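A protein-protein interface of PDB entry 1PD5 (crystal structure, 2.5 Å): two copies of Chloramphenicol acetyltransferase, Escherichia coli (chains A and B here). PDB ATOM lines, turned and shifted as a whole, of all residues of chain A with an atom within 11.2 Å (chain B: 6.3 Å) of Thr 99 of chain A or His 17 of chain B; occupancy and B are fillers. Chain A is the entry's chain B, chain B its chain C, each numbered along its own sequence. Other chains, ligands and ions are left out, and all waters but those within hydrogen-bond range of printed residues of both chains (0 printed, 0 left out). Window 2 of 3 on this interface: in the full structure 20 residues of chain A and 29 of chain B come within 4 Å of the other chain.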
ATOM      1  N   VAL A  94      23.179   0.293  -5.649  1.00  0.00           N
ATOM      2  CA  VAL A  94      23.448   0.065  -7.031  1.00  0.00           C
ATOM      3  C   VAL A  94      22.905   1.366  -7.629  1.00  0.00           C
ATOM      4  O   VAL A  94      21.732   1.773  -7.318  1.00  0.00           O
ATOM      5  CB  VAL A  94      22.706  -1.259  -7.294  1.00  0.00           C
ATOM      6  CG1 VAL A  94      21.869  -1.366  -8.530  1.00  0.00           C
ATOM      7  CG2 VAL A  94      23.719  -2.342  -7.272  1.00  0.00           C
ATOM      8  N   PHE A  95      23.772   2.058  -8.388  1.00  0.00           N
ATOM      9  CA  PHE A  95      23.511   3.394  -9.034  1.00  0.00           C
ATOM     10  C   PHE A  95      23.088   3.189 -10.469  1.00  0.00           C
ATOM     11  O   PHE A  95      23.629   2.324 -11.092  1.00  0.00           O
ATOM     12  CB  PHE A  95      24.750   4.200  -9.024  1.00  0.00           C
ATOM     13  CG  PHE A  95      24.595   5.662  -9.507  1.00  0.00           C
ATOM     14  CD1 PHE A  95      23.655   6.554  -8.908  1.00  0.00           C
ATOM     15  CD2 PHE A  95      25.453   6.177 -10.552  1.00  0.00           C
ATOM     16  CE1 PHE A  95      23.545   7.881  -9.333  1.00  0.00           C
ATOM     17  CE2 PHE A  95      25.342   7.455 -10.930  1.00  0.00           C
ATOM     18  CZ  PHE A  95      24.386   8.328 -10.291  1.00  0.00           C
ATOM     19  N   HIS A  96      22.035   3.912 -10.916  1.00  0.00           N
ATOM     20  CA  HIS A  96      21.531   3.996 -12.285  1.00  0.00           C
ATOM     21  C   HIS A  96      21.864   5.424 -12.956  1.00  0.00           C
ATOM     22  O   HIS A  96      21.149   6.430 -12.807  1.00  0.00           O
ATOM     23  CB  HIS A  96      20.028   3.796 -12.357  1.00  0.00           C
ATOM     24  CG  HIS A  96      19.476   2.724 -11.463  1.00  0.00           C
ATOM     25  ND1 HIS A  96      19.835   1.386 -11.541  1.00  0.00           N
ATOM     26  CD2 HIS A  96      18.540   2.797 -10.475  1.00  0.00           C
ATOM     27  CE1 HIS A  96      19.097   0.688 -10.689  1.00  0.00           C
ATOM     28  NE2 HIS A  96      18.344   1.526  -9.990  1.00  0.00           N
ATOM     29  N   GLU A  97      22.966   5.441 -13.707  1.00  0.00           N
ATOM     30  CA  GLU A  97      23.459   6.475 -14.626  1.00  0.00           C
ATOM     31  C   GLU A  97      22.376   7.272 -15.306  1.00  0.00           C
ATOM     32  O   GLU A  97      22.321   8.477 -15.118  1.00  0.00           O
ATOM     33  CB  GLU A  97      24.280   5.809 -15.770  1.00  0.00           C
ATOM     34  CG  GLU A  97      25.608   5.200 -15.398  1.00  0.00           C
ATOM     35  CD  GLU A  97      26.666   6.301 -15.413  1.00  0.00           C
ATOM     36  OE1 GLU A  97      26.897   6.862 -16.546  1.00  0.00           O
ATOM     37  OE2 GLU A  97      27.218   6.641 -14.308  1.00  0.00           O
ATOM     38  N   GLN A  98      21.577   6.616 -16.167  1.00  0.00           N
ATOM     39  CA  GLN A  98      20.583   7.343 -16.984  1.00  0.00           C
ATOM     40  C   GLN A  98      19.644   8.138 -16.121  1.00  0.00           C
ATOM     41  O   GLN A  98      19.409   9.258 -16.454  1.00  0.00           O
ATOM     42  CB  GLN A  98      19.795   6.496 -18.074  1.00  0.00           C
ATOM     43  CG  GLN A  98      20.667   5.503 -19.031  1.00  0.00           C
ATOM     44  CD  GLN A  98      21.382   6.238 -20.270  1.00  0.00           C
ATOM     45  OE1 GLN A  98      22.312   7.083 -20.035  1.00  0.00           O
ATOM     46  NE2 GLN A  98      20.950   5.913 -21.568  1.00  0.00           N
ATOM     47  N   THR A  99      19.117   7.646 -15.000  1.00  0.00           N
ATOM     48  CA  THR A  99      18.205   8.498 -14.255  1.00  0.00           C
ATOM     49  C   THR A  99      18.931   9.203 -13.087  1.00  0.00           C
ATOM     50  O   THR A  99      18.350  10.044 -12.352  1.00  0.00           O
ATOM     51  CB  THR A  99      17.069   7.697 -13.669  1.00  0.00           C
ATOM     52  OG1 THR A  99      17.633   6.738 -12.745  1.00  0.00           O
ATOM     53  CG2 THR A  99      16.214   6.932 -14.721  1.00  0.00           C
ATOM     54  N   GLU A 100      20.157   8.822 -12.832  1.00  0.00           N
ATOM     55  CA  GLU A 100      20.770   9.359 -11.585  1.00  0.00           C
ATOM     56  C   GLU A 100      19.927   9.031 -10.347  1.00  0.00           C
ATOM     57  O   GLU A 100      19.823   9.867  -9.436  1.00  0.00           O
ATOM     58  CB  GLU A 100      20.895  10.859 -11.699  1.00  0.00           C
ATOM     59  CG  GLU A 100      22.130  11.266 -12.520  1.00  0.00           C
ATOM     60  CD  GLU A 100      21.994  12.621 -13.219  1.00  0.00           C
ATOM     61  OE1 GLU A 100      20.966  13.322 -13.095  1.00  0.00           O
ATOM     62  OE2 GLU A 100      22.933  12.989 -13.888  1.00  0.00           O
ATOM     63  N   THR A 101      19.283   7.842 -10.323  1.00  0.00           N
ATOM     64  CA  THR A 101      18.818   7.404  -9.049  1.00  0.00           C
ATOM     65  C   THR A 101      19.599   6.183  -8.486  1.00  0.00           C
ATOM     66  O   THR A 101      20.542   5.612  -9.181  1.00  0.00           O
ATOM     67  CB  THR A 101      17.383   7.117  -9.103  1.00  0.00           C
ATOM     68  OG1 THR A 101      17.224   6.170 -10.159  1.00  0.00           O
ATOM     69  CG2 THR A 101      16.544   8.430  -9.444  1.00  0.00           C
ATOM     70  N   PHE A 102      19.266   5.794  -7.243  1.00  0.00           N
ATOM     71  CA  PHE A 102      19.802   4.550  -6.792  1.00  0.00           C
ATOM     72  C   PHE A 102      18.717   3.592  -6.344  1.00  0.00           C
ATOM     73  O   PHE A 102      17.521   4.017  -6.109  1.00  0.00           O
ATOM     74  CB  PHE A 102      20.860   4.735  -5.679  1.00  0.00           C
ATOM     75  CG  PHE A 102      20.246   5.079  -4.370  1.00  0.00           C
ATOM     76  CD1 PHE A 102      19.992   4.071  -3.457  1.00  0.00           C
ATOM     77  CD2 PHE A 102      19.829   6.413  -4.099  1.00  0.00           C
ATOM     78  CE1 PHE A 102      19.405   4.332  -2.242  1.00  0.00           C
ATOM     79  CE2 PHE A 102      19.277   6.675  -2.951  1.00  0.00           C
ATOM     80  CZ  PHE A 102      19.044   5.578  -1.947  1.00  0.00           C
ATOM     81  N   SER A 103      19.161   2.324  -6.287  1.00  0.00           N
ATOM     82  CA  SER A 103      18.372   1.226  -5.723  1.00  0.00           C
ATOM     83  C   SER A 103      19.212   0.518  -4.627  1.00  0.00           C
ATOM     84  O   SER A 103      20.451   0.613  -4.612  1.00  0.00           O
ATOM     85  CB  SER A 103      17.877   0.148  -6.723  1.00  0.00           C
ATOM     86  OG  SER A 103      17.370   0.688  -7.920  1.00  0.00           O
ATOM     87  N   TYR A 127      18.507  -7.388 -11.645  1.00  0.00           N
ATOM     88  CA  TYR A 127      17.825  -6.318 -10.914  1.00  0.00           C
ATOM     89  C   TYR A 127      18.571  -4.993 -11.073  1.00  0.00           C
ATOM     90  O   TYR A 127      17.977  -3.977 -10.726  1.00  0.00           O
ATOM     91  CB  TYR A 127      17.634  -6.676  -9.466  1.00  0.00           C
ATOM     92  CG  TYR A 127      16.703  -7.767  -9.230  1.00  0.00           C
ATOM     93  CD1 TYR A 127      15.413  -7.591  -9.468  1.00  0.00           C
ATOM     94  CD2 TYR A 127      17.087  -8.990  -8.736  1.00  0.00           C
ATOM     95  CE1 TYR A 127      14.524  -8.556  -9.275  1.00  0.00           C
ATOM     96  CE2 TYR A 127      16.126 -10.042  -8.548  1.00  0.00           C
ATOM     97  CZ  TYR A 127      14.829  -9.768  -8.826  1.00  0.00           C
ATOM     98  OH  TYR A 127      13.695 -10.685  -8.655  1.00  0.00           O
ATOM     99  N   GLY A 128      19.813  -5.022 -11.653  1.00  0.00           N
ATOM    100  CA  GLY A 128      20.743  -3.868 -11.754  1.00  0.00           C
ATOM    101  C   GLY A 128      20.084  -2.682 -12.412  1.00  0.00           C
ATOM    102  O   GLY A 128      20.437  -1.552 -12.150  1.00  0.00           O
ATOM    103  N   GLU A 129      19.002  -2.927 -13.129  1.00  0.00           N
ATOM    104  CA  GLU A 129      18.412  -1.970 -14.077  1.00  0.00           C
ATOM    105  C   GLU A 129      16.956  -1.575 -13.654  1.00  0.00           C
ATOM    106  O   GLU A 129      16.271  -0.676 -14.194  1.00  0.00           O
ATOM    107  CB  GLU A 129      18.336  -2.662 -15.472  1.00  0.00           C
ATOM    108  CG  GLU A 129      19.024  -1.907 -16.625  1.00  0.00           C
ATOM    109  CD  GLU A 129      20.569  -1.809 -16.489  1.00  0.00           C
ATOM    110  OE1 GLU A 129      21.145  -0.960 -17.228  1.00  0.00           O
ATOM    111  OE2 GLU A 129      21.192  -2.555 -15.665  1.00  0.00           O
ATOM    112  N   ASN A 130      16.469  -2.334 -12.723  1.00  0.00           N
ATOM    113  CA  ASN A 130      15.192  -2.068 -12.213  1.00  0.00           C
ATOM    114  C   ASN A 130      15.271  -0.754 -11.440  1.00  0.00           C
ATOM    115  O   ASN A 130      16.040  -0.595 -10.457  1.00  0.00           O
ATOM    116  CB  ASN A 130      14.879  -3.237 -11.288  1.00  0.00           C
ATOM    117  CG  ASN A 130      13.494  -3.249 -10.854  1.00  0.00           C
ATOM    118  OD1 ASN A 130      12.927  -2.187 -10.489  1.00  0.00           O
ATOM    119  ND2 ASN A 130      12.855  -4.423 -10.983  1.00  0.00           N
ATOM    120  N   LEU A 131      14.480   0.194 -11.847  1.00  0.00           N
ATOM    121  CA  LEU A 131      14.436   1.450 -11.066  1.00  0.00           C
ATOM    122  C   LEU A 131      13.616   1.499  -9.705  1.00  0.00           C
ATOM    123  O   LEU A 131      13.595   2.566  -9.051  1.00  0.00           O
ATOM    124  CB  LEU A 131      14.086   2.615 -11.958  1.00  0.00           C
ATOM    125  CG  LEU A 131      14.829   2.625 -13.282  1.00  0.00           C
ATOM    126  CD1 LEU A 131      13.962   3.489 -14.195  1.00  0.00           C
ATOM    127  CD2 LEU A 131      16.246   3.146 -13.226  1.00  0.00           C
ATOM    128  N   ALA A 132      12.990   0.398  -9.270  1.00  0.00           N
ATOM    129  CA  ALA A 132      12.304   0.422  -7.974  1.00  0.00           C
ATOM    130  C   ALA A 132      13.361   0.753  -6.962  1.00  0.00           C
ATOM    131  O   ALA A 132      14.577   0.515  -7.182  1.00  0.00           O
ATOM    132  CB  ALA A 132      11.580  -0.965  -7.593  1.00  0.00           C
ATOM    133  N   TYR A 133      12.946   1.297  -5.834  1.00  0.00           N
ATOM    134  CA  TYR A 133      13.907   1.493  -4.724  1.00  0.00           C
ATOM    135  C   TYR A 133      14.598   0.124  -4.158  1.00  0.00           C
ATOM    136  O   TYR A 133      15.858  -0.023  -3.949  1.00  0.00           O
ATOM    137  CB  TYR A 133      13.162   2.337  -3.694  1.00  0.00           C
ATOM    138  CG  TYR A 133      13.888   2.703  -2.467  1.00  0.00           C
ATOM    139  CD1 TYR A 133      15.285   2.672  -2.414  1.00  0.00           C
ATOM    140  CD2 TYR A 133      13.174   3.203  -1.316  1.00  0.00           C
ATOM    141  CE1 TYR A 133      15.970   3.093  -1.229  1.00  0.00           C
ATOM    142  CE2 TYR A 133      13.858   3.543  -0.157  1.00  0.00           C
ATOM    143  CZ  TYR A 133      15.277   3.435  -0.134  1.00  0.00           C
ATOM    144  OH  TYR A 133      16.012   3.709   1.020  1.00  0.00           O
ATOM    145  N   PHE A 134      13.702  -0.808  -3.874  1.00  0.00           N
ATOM    146  CA  PHE A 134      13.973  -2.151  -3.383  1.00  0.00           C
ATOM    147  C   PHE A 134      13.471  -3.085  -4.446  1.00  0.00           C
ATOM    148  O   PHE A 134      12.369  -3.609  -4.373  1.00  0.00           O
ATOM    149  CB  PHE A 134      13.214  -2.385  -2.061  1.00  0.00           C
ATOM    150  CG  PHE A 134      13.996  -1.873  -0.878  1.00  0.00           C
ATOM    151  CD1 PHE A 134      13.708  -0.603  -0.332  1.00  0.00           C
ATOM    152  CD2 PHE A 134      15.107  -2.611  -0.375  1.00  0.00           C
ATOM    153  CE1 PHE A 134      14.528  -0.075   0.720  1.00  0.00           C
ATOM    154  CE2 PHE A 134      15.900  -2.119   0.727  1.00  0.00           C
ATOM    155  CZ  PHE A 134      15.616  -0.809   1.243  1.00  0.00           C
ATOM    156  N   TRP A 150      32.209   8.959  -5.158  1.00  0.00           N
ATOM    157  CA  TRP A 150      32.512  10.307  -5.669  1.00  0.00           C
ATOM    158  C   TRP A 150      33.463  10.882  -4.718  1.00  0.00           C
ATOM    159  O   TRP A 150      34.219  11.780  -5.008  1.00  0.00           O
ATOM    160  CB  TRP A 150      31.233  11.119  -5.667  1.00  0.00           C
ATOM    161  CG  TRP A 150      30.238  10.428  -6.472  1.00  0.00           C
ATOM    162  CD1 TRP A 150      30.197  10.365  -7.837  1.00  0.00           C
ATOM    163  CD2 TRP A 150      29.209   9.592  -6.012  1.00  0.00           C
ATOM    164  NE1 TRP A 150      29.201   9.542  -8.250  1.00  0.00           N
ATOM    165  CE2 TRP A 150      28.585   9.025  -7.148  1.00  0.00           C
ATOM    166  CE3 TRP A 150      28.721   9.256  -4.739  1.00  0.00           C
ATOM    167  CZ2 TRP A 150      27.523   8.153  -7.067  1.00  0.00           C
ATOM    168  CZ3 TRP A 150      27.621   8.369  -4.662  1.00  0.00           C
ATOM    169  CH2 TRP A 150      27.021   7.873  -5.841  1.00  0.00           C
ATOM    170  N   ILE B  13       5.380  15.015  -8.514  1.00  0.00           N
ATOM    171  CA  ILE B  13       5.890  13.895  -7.779  1.00  0.00           C
ATOM    172  C   ILE B  13       5.735  12.660  -8.700  1.00  0.00           C
ATOM    173  O   ILE B  13       6.588  11.833  -8.878  1.00  0.00           O
ATOM    174  CB  ILE B  13       4.958  13.684  -6.547  1.00  0.00           C
ATOM    175  CG1 ILE B  13       4.420  15.044  -5.953  1.00  0.00           C
ATOM    176  CG2 ILE B  13       5.552  12.626  -5.579  1.00  0.00           C
ATOM    177  CD1 ILE B  13       3.054  15.865  -6.854  1.00  0.00           C
ATOM    178  N   GLN B  15       5.856  12.079 -11.608  1.00  0.00           N
ATOM    179  CA  GLN B  15       6.687  11.775 -12.763  1.00  0.00           C
ATOM    180  C   GLN B  15       8.130  11.927 -12.318  1.00  0.00           C
ATOM    181  O   GLN B  15       9.043  11.977 -13.170  1.00  0.00           O
ATOM    182  CB  GLN B  15       6.393  12.731 -13.932  1.00  0.00           C
ATOM    183  CG  GLN B  15       4.823  12.884 -14.346  1.00  0.00           C
ATOM    184  CD  GLN B  15       4.078  11.449 -14.702  1.00  0.00           C
ATOM    185  OE1 GLN B  15       4.648  10.619 -15.494  1.00  0.00           O
ATOM    186  NE2 GLN B  15       2.856  11.173 -14.062  1.00  0.00           N
ATOM    187  N   TRP B  16       8.373  11.997 -10.993  1.00  0.00           N
ATOM    188  CA  TRP B  16       9.706  12.178 -10.532  1.00  0.00           C
ATOM    189  C   TRP B  16      10.377  10.809 -10.381  1.00  0.00           C
ATOM    190  O   TRP B  16       9.770   9.906  -9.731  1.00  0.00           O
ATOM    191  CB  TRP B  16       9.633  12.834  -9.227  1.00  0.00           C
ATOM    192  CG  TRP B  16      10.928  13.315  -8.630  1.00  0.00           C
ATOM    193  CD1 TRP B  16      12.154  13.545  -9.239  1.00  0.00           C
ATOM    194  CD2 TRP B  16      11.088  13.695  -7.258  1.00  0.00           C
ATOM    195  NE1 TRP B  16      13.046  14.044  -8.306  1.00  0.00           N
ATOM    196  CE2 TRP B  16      12.428  14.137  -7.090  1.00  0.00           C
ATOM    197  CE3 TRP B  16      10.236  13.689  -6.157  1.00  0.00           C
ATOM    198  CZ2 TRP B  16      12.892  14.595  -5.909  1.00  0.00           C
ATOM    199  CZ3 TRP B  16      10.736  14.147  -4.948  1.00  0.00           C
ATOM    200  CH2 TRP B  16      12.042  14.579  -4.831  1.00  0.00           C
ATOM    201  N   HIS B  17      11.599  10.666 -10.979  1.00  0.00           N
ATOM    202  CA  HIS B  17      12.331   9.427 -10.871  1.00  0.00           C
ATOM    203  C   HIS B  17      12.601   9.088  -9.448  1.00  0.00           C
ATOM    204  O   HIS B  17      12.748   7.947  -9.177  1.00  0.00           O
ATOM    205  CB  HIS B  17      13.659   9.404 -11.626  1.00  0.00           C
ATOM    206  CG  HIS B  17      13.520   9.479 -13.118  1.00  0.00           C
ATOM    207  ND1 HIS B  17      12.644   8.679 -13.838  1.00  0.00           N
ATOM    208  CD2 HIS B  17      14.125  10.297 -14.032  1.00  0.00           C
ATOM    209  CE1 HIS B  17      12.740   8.979 -15.127  1.00  0.00           C
ATOM    210  NE2 HIS B  17      13.629   9.953 -15.274  1.00  0.00           N
ATOM    211  N   ARG B  18      12.663  10.063  -8.525  1.00  0.00           N
ATOM    212  CA  ARG B  18      12.819   9.796  -7.082  1.00  0.00           C
ATOM    213  C   ARG B  18      11.513   9.765  -6.240  1.00  0.00           C
ATOM    214  O   ARG B  18      11.580   9.779  -5.006  1.00  0.00           O
ATOM    215  CB  ARG B  18      13.853  10.737  -6.447  1.00  0.00           C
ATOM    216  CG  ARG B  18      15.310  10.559  -6.941  1.00  0.00           C
ATOM    217  CD  ARG B  18      16.232  11.542  -6.255  1.00  0.00           C
ATOM    218  NE  ARG B  18      16.480  11.319  -4.815  1.00  0.00           N
ATOM    219  CZ  ARG B  18      15.864  11.953  -3.788  1.00  0.00           C
ATOM    220  NH1 ARG B  18      14.849  12.894  -3.902  1.00  0.00           N
ATOM    221  NH2 ARG B  18      16.221  11.559  -2.587  1.00  0.00           N
ATOM    222  N   LYS B  19      10.348   9.716  -6.870  1.00  0.00           N
ATOM    223  CA  LYS B  19       9.083   9.494  -6.167  1.00  0.00           C
ATOM    224  C   LYS B  19       9.176   8.566  -4.954  1.00  0.00           C
ATOM    225  O   LYS B  19       8.840   8.987  -3.827  1.00  0.00           O
ATOM    226  CB  LYS B  19       8.036   8.866  -7.106  1.00  0.00           C
ATOM    227  CG  LYS B  19       6.686   9.033  -6.521  1.00  0.00           C
ATOM    228  CD  LYS B  19       5.569   8.237  -7.231  1.00  0.00           C
ATOM    229  CE  LYS B  19       4.372   8.084  -6.161  1.00  0.00           C
ATOM    230  NZ  LYS B  19       4.115   6.651  -5.566  1.00  0.00           N
ATOM    231  N   GLU B  20       9.577   7.301  -5.156  1.00  0.00           N
ATOM    232  CA  GLU B  20       9.696   6.322  -4.007  1.00  0.00           C
ATOM    233  C   GLU B  20      10.754   6.657  -2.920  1.00  0.00           C
ATOM    234  O   GLU B  20      10.473   6.419  -1.744  1.00  0.00           O
ATOM    235  CB  GLU B  20      10.023   4.878  -4.396  1.00  0.00           C
ATOM    236  CG  GLU B  20       9.013   4.116  -5.210  1.00  0.00           C
ATOM    237  CD  GLU B  20       9.549   2.728  -5.689  1.00  0.00           C
ATOM    238  OE1 GLU B  20       8.953   2.195  -6.680  1.00  0.00           O
ATOM    239  OE2 GLU B  20      10.479   2.172  -5.094  1.00  0.00           O
ATOM    240  N   HIS B  21      11.943   7.143  -3.322  1.00  0.00           N
ATOM    241  CA  HIS B  21      12.908   7.573  -2.344  1.00  0.00           C
ATOM    242  C   HIS B  21      12.380   8.742  -1.544  1.00  0.00           C
ATOM    243  O   HIS B  21      12.487   8.734  -0.357  1.00  0.00           O
ATOM    244  CB  HIS B  21      14.187   7.951  -3.016  1.00  0.00           C
ATOM    245  CG  HIS B  21      14.603   6.976  -4.049  1.00  0.00           C
ATOM    246  ND1 HIS B  21      13.939   6.855  -5.265  1.00  0.00           N
ATOM    247  CD2 HIS B  21      15.566   6.017  -4.037  1.00  0.00           C
ATOM    248  CE1 HIS B  21      14.540   5.940  -5.993  1.00  0.00           C
ATOM    249  NE2 HIS B  21      15.526   5.413  -5.274  1.00  0.00           N
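Among the printed residues, pairs that only touch across the chains: Thr 101 of chain A with Arg 18 of chain B, Ala 132 of chain A with Glu 20 of chain B, Tyr 133 of chain A with His 21 of chain B, Thr 101 of chain A with His 17 of chain B and Thr 99 of chain A with His 17 of chain B.
The backbone NH (N) of Tyr 133 of chain A is in hydrogen-bond range of the side-chain carboxylate (OE2) of Glu 20 of chain B, 2.7 Å away. The backbone carbonyl oxygen (O) of Phe 102 of chain A sits at hydrogen-bond distance from a ring nitrogen (NE2) of His 21 of chain B, 2.6 Å away.
Gln 98 of chain A touches none of the printed residues of chain B. Thr 99 of chain A touches just one residue of chain B: His 17. Of the printed residues of chain B, Phe 102 of chain A touches His 21. Printed residues of chain B within 4 Å of Tyr 133 of chain A: Glu 20 (2.7 Å) and His 21 (3.7 Å). Trp 16 of chain B touches none of the printed residues of chain A. His 17 of chain B touches just these residues of chain A: Thr 99 and Thr 101. Printed residues of chain A within 4 Å of Arg 18 of chain B: Thr 101. Printed residues of chain A within 4 Å of Glu 20 of chain B: Ala 132 (3.7 Å) and Tyr 133 (2.7 Å). Of the printed residues of chain A, His 21 of chain B touches Phe 102 (2.6 Å) and Tyr 133 (3.7 Å). The nearest printed residue of chain B that does not touch Thr 101 of chain A is His 21 of chain B (4.4 Å).
No position is printed for both chains. Of the 7 pairs that touch across the chains among the printed residues, none has its exchanged pair printed and touching as well.
Of the 19 printed residues of chain A, 5 touch a printed residue of chain B. Of the 8 printed residues of chain B, 4 touch a printed residue of chain A. Printed residues of chain B that touch a printed residue of chain A: His 17, Arg 18, Glu 20 and His 21. Among the printed residues, 7 pairs touch across the chains.
The side-chain hydroxyl (OG1) of Thr 101 of chain A lies within hydrogen-bond range of the side-chain hydroxyl (OG1) of Thr 99 of chain A (2.7 Å). The backbone NH (N) of His 96 of chain A is in hydrogen-bond range of the backbone carbonyl oxygen (O) of Thr 101 of chain A, at 2.9 Å. The backbone carbonyl oxygen of Ala 132 of chain A is in hydrogen-bond range of the side-chain hydroxyl of Ser 103 of chain A (2.9 Å). The side-chain amide oxygen (OD1) of Asn 130 of chain A lies within hydrogen-bond range of the backbone NH (N) of Ala 132 of chain A, 2.9 Å away.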
